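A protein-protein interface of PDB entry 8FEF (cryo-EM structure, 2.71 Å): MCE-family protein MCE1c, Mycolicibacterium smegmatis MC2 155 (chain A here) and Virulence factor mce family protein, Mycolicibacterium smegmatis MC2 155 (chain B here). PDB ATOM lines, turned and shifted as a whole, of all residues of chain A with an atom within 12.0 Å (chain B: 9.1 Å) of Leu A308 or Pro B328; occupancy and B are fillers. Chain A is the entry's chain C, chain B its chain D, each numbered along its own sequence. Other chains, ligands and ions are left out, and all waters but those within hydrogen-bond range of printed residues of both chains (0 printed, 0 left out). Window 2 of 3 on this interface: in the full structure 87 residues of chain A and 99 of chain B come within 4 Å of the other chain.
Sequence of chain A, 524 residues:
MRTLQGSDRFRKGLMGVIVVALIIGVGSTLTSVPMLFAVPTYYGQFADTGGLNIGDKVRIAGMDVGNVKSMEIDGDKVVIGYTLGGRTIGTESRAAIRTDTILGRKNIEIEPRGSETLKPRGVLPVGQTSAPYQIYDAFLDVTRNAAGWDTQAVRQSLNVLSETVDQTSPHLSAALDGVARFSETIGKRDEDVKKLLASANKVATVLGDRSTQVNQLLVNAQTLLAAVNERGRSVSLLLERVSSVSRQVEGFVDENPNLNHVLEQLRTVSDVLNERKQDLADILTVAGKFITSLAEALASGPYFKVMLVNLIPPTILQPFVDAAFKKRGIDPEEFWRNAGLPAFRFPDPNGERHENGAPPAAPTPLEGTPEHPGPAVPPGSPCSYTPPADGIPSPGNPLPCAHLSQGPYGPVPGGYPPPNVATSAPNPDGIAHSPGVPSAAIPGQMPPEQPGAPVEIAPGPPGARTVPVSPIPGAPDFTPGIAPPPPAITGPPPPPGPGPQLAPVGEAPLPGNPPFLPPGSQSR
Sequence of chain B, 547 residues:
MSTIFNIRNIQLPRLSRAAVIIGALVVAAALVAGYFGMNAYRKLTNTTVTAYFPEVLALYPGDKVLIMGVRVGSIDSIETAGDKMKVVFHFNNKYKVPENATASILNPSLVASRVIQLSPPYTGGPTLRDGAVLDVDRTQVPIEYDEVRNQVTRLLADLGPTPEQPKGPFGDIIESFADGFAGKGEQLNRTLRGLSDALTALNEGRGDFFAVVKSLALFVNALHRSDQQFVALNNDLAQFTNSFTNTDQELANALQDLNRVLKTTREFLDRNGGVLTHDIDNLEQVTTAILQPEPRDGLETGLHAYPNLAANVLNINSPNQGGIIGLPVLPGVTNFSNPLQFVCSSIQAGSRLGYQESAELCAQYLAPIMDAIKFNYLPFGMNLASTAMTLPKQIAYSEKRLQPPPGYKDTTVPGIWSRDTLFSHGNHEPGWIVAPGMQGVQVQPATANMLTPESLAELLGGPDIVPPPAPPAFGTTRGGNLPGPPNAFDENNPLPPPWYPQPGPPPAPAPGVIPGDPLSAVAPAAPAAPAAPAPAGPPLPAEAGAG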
ATOM      1  N   ALA A 297     -21.865  23.311  -2.660  1.00  0.00           N
ATOM      2  CA  ALA A 297     -21.726  22.524  -1.442  1.00  0.00           C
ATOM      3  C   ALA A 297     -21.917  23.383  -0.220  1.00  0.00           C
ATOM      4  O   ALA A 297     -22.553  22.971   0.729  1.00  0.00           O
ATOM      5  CB  ALA A 297     -20.369  21.861  -1.405  1.00  0.00           C
ATOM      6  N   SER A 300     -26.227  24.564   1.133  1.00  0.00           N
ATOM      7  CA  SER A 300     -27.293  23.870   1.863  1.00  0.00           C
ATOM      8  C   SER A 300     -27.492  24.253   3.316  1.00  0.00           C
ATOM      9  O   SER A 300     -28.608  24.243   3.772  1.00  0.00           O
ATOM     10  CB  SER A 300     -27.117  22.351   1.775  1.00  0.00           C
ATOM     11  OG  SER A 300     -26.874  21.915   0.446  1.00  0.00           O
ATOM     12  N   GLY A 301     -26.426  24.527   4.055  1.00  0.00           N
ATOM     13  CA  GLY A 301     -26.503  24.886   5.469  1.00  0.00           C
ATOM     14  C   GLY A 301     -25.263  25.664   5.873  1.00  0.00           C
ATOM     15  O   GLY A 301     -24.469  26.013   5.020  1.00  0.00           O
ATOM     16  N   PRO A 302     -25.091  25.995   7.164  1.00  0.00           N
ATOM     17  CA  PRO A 302     -23.856  26.710   7.532  1.00  0.00           C
ATOM     18  C   PRO A 302     -22.650  25.782   7.765  1.00  0.00           C
ATOM     19  O   PRO A 302     -22.170  25.682   8.880  1.00  0.00           O
ATOM     20  CB  PRO A 302     -24.235  27.400   8.839  1.00  0.00           C
ATOM     21  CG  PRO A 302     -25.296  26.546   9.418  1.00  0.00           C
ATOM     22  CD  PRO A 302     -26.028  25.883   8.287  1.00  0.00           C
ATOM     23  N   TYR A 303     -22.177  25.146   6.692  1.00  0.00           N
ATOM     24  CA  TYR A 303     -21.076  24.184   6.649  1.00  0.00           C
ATOM     25  C   TYR A 303     -20.878  23.838   5.175  1.00  0.00           C
ATOM     26  O   TYR A 303     -21.125  24.664   4.326  1.00  0.00           O
ATOM     27  CB  TYR A 303     -21.451  22.911   7.417  1.00  0.00           C
ATOM     28  CG  TYR A 303     -22.886  22.443   7.236  1.00  0.00           C
ATOM     29  CD1 TYR A 303     -23.292  21.824   6.073  1.00  0.00           C
ATOM     30  CD2 TYR A 303     -23.826  22.632   8.228  1.00  0.00           C
ATOM     31  CE1 TYR A 303     -24.593  21.410   5.899  1.00  0.00           C
ATOM     32  CE2 TYR A 303     -25.130  22.228   8.060  1.00  0.00           C
ATOM     33  CZ  TYR A 303     -25.502  21.615   6.893  1.00  0.00           C
ATOM     34  OH  TYR A 303     -26.797  21.205   6.721  1.00  0.00           O
ATOM     35  N   PHE A 304     -20.386  22.643   4.870  1.00  0.00           N
ATOM     36  CA  PHE A 304     -20.266  22.152   3.504  1.00  0.00           C
ATOM     37  C   PHE A 304     -20.406  20.638   3.502  1.00  0.00           C
ATOM     38  O   PHE A 304     -19.885  19.960   4.389  1.00  0.00           O
ATOM     39  CB  PHE A 304     -18.935  22.572   2.857  1.00  0.00           C
ATOM     40  CG  PHE A 304     -17.715  22.184   3.645  1.00  0.00           C
ATOM     41  CD1 PHE A 304     -17.200  23.034   4.600  1.00  0.00           C
ATOM     42  CD2 PHE A 304     -17.067  20.985   3.410  1.00  0.00           C
ATOM     43  CE1 PHE A 304     -16.077  22.688   5.319  1.00  0.00           C
ATOM     44  CE2 PHE A 304     -15.944  20.638   4.132  1.00  0.00           C
ATOM     45  CZ  PHE A 304     -15.451  21.488   5.084  1.00  0.00           C
ATOM     46  N   LYS A 305     -21.119  20.110   2.516  1.00  0.00           N
ATOM     47  CA  LYS A 305     -21.265  18.667   2.419  1.00  0.00           C
ATOM     48  C   LYS A 305     -19.970  18.030   1.930  1.00  0.00           C
ATOM     49  O   LYS A 305     -19.238  18.602   1.119  1.00  0.00           O
ATOM     50  CB  LYS A 305     -22.409  18.308   1.476  1.00  0.00           C
ATOM     51  CG  LYS A 305     -23.737  18.928   1.848  1.00  0.00           C
ATOM     52  CD  LYS A 305     -24.842  18.414   0.947  1.00  0.00           C
ATOM     53  CE  LYS A 305     -26.123  19.186   1.170  1.00  0.00           C
ATOM     54  NZ  LYS A 305     -26.450  19.260   2.615  1.00  0.00           N
ATOM     55  N   VAL A 306     -19.688  16.835   2.440  1.00  0.00           N
ATOM     56  CA  VAL A 306     -18.518  16.061   2.044  1.00  0.00           C
ATOM     57  C   VAL A 306     -18.917  14.601   1.901  1.00  0.00           C
ATOM     58  O   VAL A 306     -19.683  14.072   2.712  1.00  0.00           O
ATOM     59  CB  VAL A 306     -17.356  16.206   3.047  1.00  0.00           C
ATOM     60  CG1 VAL A 306     -16.676  17.532   2.868  1.00  0.00           C
ATOM     61  CG2 VAL A 306     -17.856  16.065   4.472  1.00  0.00           C
ATOM     62  N   MET A 307     -18.405  13.952   0.862  1.00  0.00           N
ATOM     63  CA  MET A 307     -18.611  12.527   0.650  1.00  0.00           C
ATOM     64  C   MET A 307     -17.326  11.794   1.008  1.00  0.00           C
ATOM     65  O   MET A 307     -16.297  11.981   0.351  1.00  0.00           O
ATOM     66  CB  MET A 307     -19.014  12.230  -0.792  1.00  0.00           C
ATOM     67  CG  MET A 307     -19.467  10.797  -1.005  1.00  0.00           C
ATOM     68  SD  MET A 307     -19.896  10.419  -2.711  1.00  0.00           S
ATOM     69  CE  MET A 307     -20.649   8.809  -2.511  1.00  0.00           C
ATOM     70  N   LEU A 308     -17.390  10.962   2.041  1.00  0.00           N
ATOM     71  CA  LEU A 308     -16.244  10.198   2.516  1.00  0.00           C
ATOM     72  C   LEU A 308     -16.356   8.786   1.954  1.00  0.00           C
ATOM     73  O   LEU A 308     -17.173   7.989   2.422  1.00  0.00           O
ATOM     74  CB  LEU A 308     -16.200  10.186   4.041  1.00  0.00           C
ATOM     75  CG  LEU A 308     -16.267  11.555   4.722  1.00  0.00           C
ATOM     76  CD1 LEU A 308     -16.544  11.404   6.207  1.00  0.00           C
ATOM     77  CD2 LEU A 308     -14.977  12.317   4.499  1.00  0.00           C
ATOM     78  N   VAL A 309     -15.534   8.479   0.947  1.00  0.00           N
ATOM     79  CA  VAL A 309     -15.565   7.162   0.324  1.00  0.00           C
ATOM     80  C   VAL A 309     -14.949   6.092   1.218  1.00  0.00           C
ATOM     81  O   VAL A 309     -15.137   4.893   0.977  1.00  0.00           O
ATOM     82  CB  VAL A 309     -14.873   7.300  -1.055  1.00  0.00           C
ATOM     83  CG1 VAL A 309     -14.725   5.969  -1.787  1.00  0.00           C
ATOM     84  CG2 VAL A 309     -15.630   8.292  -1.918  1.00  0.00           C
ATOM     85  N   ASN A 310     -14.296   6.493   2.304  1.00  0.00           N
ATOM     86  CA  ASN A 310     -13.740   5.538   3.254  1.00  0.00           C
ATOM     87  C   ASN A 310     -14.419   5.650   4.616  1.00  0.00           C
ATOM     88  O   ASN A 310     -13.876   6.243   5.548  1.00  0.00           O
ATOM     89  CB  ASN A 310     -12.235   5.748   3.392  1.00  0.00           C
ATOM     90  CG  ASN A 310     -11.509   5.574   2.080  1.00  0.00           C
ATOM     91  OD1 ASN A 310     -11.982   4.874   1.187  1.00  0.00           O
ATOM     92  ND2 ASN A 310     -10.356   6.213   1.952  1.00  0.00           N
ATOM     93  N   ILE B 325     -16.450  23.477   9.142  1.00  0.00           N
ATOM     94  CA  ILE B 325     -17.395  22.452   9.567  1.00  0.00           C
ATOM     95  C   ILE B 325     -17.980  21.793   8.329  1.00  0.00           C
ATOM     96  O   ILE B 325     -18.424  22.483   7.405  1.00  0.00           O
ATOM     97  CB  ILE B 325     -18.511  23.044  10.447  1.00  0.00           C
ATOM     98  CG1 ILE B 325     -17.914  23.744  11.664  1.00  0.00           C
ATOM     99  CG2 ILE B 325     -19.483  21.965  10.887  1.00  0.00           C
ATOM    100  CD1 ILE B 325     -18.942  24.425  12.523  1.00  0.00           C
ATOM    101  N   GLY B 326     -17.994  20.466   8.317  1.00  0.00           N
ATOM    102  CA  GLY B 326     -18.560  19.718   7.213  1.00  0.00           C
ATOM    103  C   GLY B 326     -19.304  18.491   7.689  1.00  0.00           C
ATOM    104  O   GLY B 326     -18.858  17.838   8.635  1.00  0.00           O
ATOM    105  N   LEU B 327     -20.428  18.149   7.058  1.00  0.00           N
ATOM    106  CA  LEU B 327     -21.092  16.966   7.567  1.00  0.00           C
ATOM    107  C   LEU B 327     -21.099  15.844   6.536  1.00  0.00           C
ATOM    108  O   LEU B 327     -21.246  16.096   5.336  1.00  0.00           O
ATOM    109  CB  LEU B 327     -22.532  17.296   8.020  1.00  0.00           C
ATOM    110  CG  LEU B 327     -23.652  17.822   7.116  1.00  0.00           C
ATOM    111  CD1 LEU B 327     -24.328  16.734   6.297  1.00  0.00           C
ATOM    112  CD2 LEU B 327     -24.676  18.533   7.980  1.00  0.00           C
ATOM    113  N   PRO B 328     -20.948  14.592   6.981  1.00  0.00           N
ATOM    114  CA  PRO B 328     -20.790  13.464   6.050  1.00  0.00           C
ATOM    115  C   PRO B 328     -22.081  12.957   5.423  1.00  0.00           C
ATOM    116  O   PRO B 328     -22.705  12.035   5.957  1.00  0.00           O
ATOM    117  CB  PRO B 328     -20.144  12.386   6.929  1.00  0.00           C
ATOM    118  CG  PRO B 328     -20.622  12.692   8.300  1.00  0.00           C
ATOM    119  CD  PRO B 328     -20.746  14.186   8.384  1.00  0.00           C
ATOM    120  N   VAL B 329     -22.502  13.555   4.304  1.00  0.00           N
ATOM    121  CA  VAL B 329     -23.682  13.052   3.609  1.00  0.00           C
ATOM    122  C   VAL B 329     -23.431  11.624   3.122  1.00  0.00           C
ATOM    123  O   VAL B 329     -22.288  11.182   2.948  1.00  0.00           O
ATOM    124  CB  VAL B 329     -24.071  13.968   2.438  1.00  0.00           C
ATOM    125  CG1 VAL B 329     -24.114  15.408   2.895  1.00  0.00           C
ATOM    126  CG2 VAL B 329     -23.104  13.799   1.278  1.00  0.00           C
ATOM    127  N   LEU B 330     -24.524  10.891   2.905  1.00  0.00           N
ATOM    128  CA  LEU B 330     -24.466   9.493   2.475  1.00  0.00           C
ATOM    129  C   LEU B 330     -25.349   9.302   1.244  1.00  0.00           C
ATOM    130  O   LEU B 330     -26.511   8.891   1.339  1.00  0.00           O
ATOM    131  CB  LEU B 330     -24.792   8.561   3.654  1.00  0.00           C
ATOM    132  CG  LEU B 330     -26.056   8.405   4.525  1.00  0.00           C
ATOM    133  CD1 LEU B 330     -27.194   7.577   3.933  1.00  0.00           C
ATOM    134  CD2 LEU B 330     -25.672   7.864   5.897  1.00  0.00           C
ATOM    135  N   PRO B 331     -24.833   9.633   0.058  1.00  0.00           N
ATOM    136  CA  PRO B 331     -25.598   9.397  -1.173  1.00  0.00           C
ATOM    137  C   PRO B 331     -25.615   7.929  -1.565  1.00  0.00           C
ATOM    138  O   PRO B 331     -25.114   7.076  -0.827  1.00  0.00           O
ATOM    139  CB  PRO B 331     -24.859  10.244  -2.218  1.00  0.00           C
ATOM    140  CG  PRO B 331     -23.956  11.150  -1.438  1.00  0.00           C
ATOM    141  CD  PRO B 331     -23.606  10.401  -0.202  1.00  0.00           C
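Ile B325 touches Tyr A303. Tyr A303 touches Leu B327 (CZ to CD2, 3.4 Å). CA of Gly B326 touches O of Phe A304, at 3.1 Å. Lys A305 touches Leu B327 (CA to O, 3.9 Å). Lys A305 touches Val B329 (CB to CG1, 3.7 Å). CA of Pro B328 touches O of Val A306, 3.6 Å away. Pro B328 touches Leu A308.
Gly A301 touches none of the printed residues of chain B. Of the printed residues of chain B, Tyr A303 touches Ile B325 (3.1 Å) and Leu B327 (3.4 Å). Printed residues of chain B within 4 Å of Val A306: Leu B327, Pro B328 and Val B329. Leu A308 touches just one residue of chain B: Pro B328 (3.8 Å). No residue of chain B comes within 4 Å of Val A309. Of the printed residues of chain A, Ile B325 touches Tyr A303 and Phe A304. Of chain A, only Phe A304 comes within 4 Å of Gly B326. Pro B328 touches just these residues of chain A: Val A306 and Leu A308. Of chain A, only Lys A305 (3.7 Å) and Val A306 (3.3 Å) come within 4 Å of Val B329. The nearest residue of chain A that does not touch Pro B328 is Met A307 (5.7 Å).
The backbone carbonyl oxygen of Ile B325 sits close to the backbone NH of Phe A304. The backbone NH (N) of Leu B327 sits at hydrogen-bond distance from the backbone carbonyl oxygen (O) of Phe A304 (3.3 Å). The backbone NH of Val A306 lies within hydrogen-bond range of the backbone carbonyl oxygen of Leu B327, 3.4 Å away. N of Val B329 sits at hydrogen-bond distance from O of Val A306 (3.3 Å).
The side-chain amino group of Lys A305 sits close to the side-chain hydroxyl of Ser A300.
Hydrophobic or aromatic side chains of chain B within 4 Å of the printed part of chain A: Leu B327, Pro B328 and Val B329. Of the 12 printed residues of chain A, 5 touch a printed residue of chain B. Hydrophobic or aromatic side chains of chain A within 4 Å of the printed part of chain B: Tyr A303, Phe A304, Val A306 and Leu A308. Among the printed residues, 11 pairs touch across the chains. Among the printed residues, no Asp or Glu carboxylate lies within 4 Å of a Lys or Arg side-chain nitrogen of the other chain.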
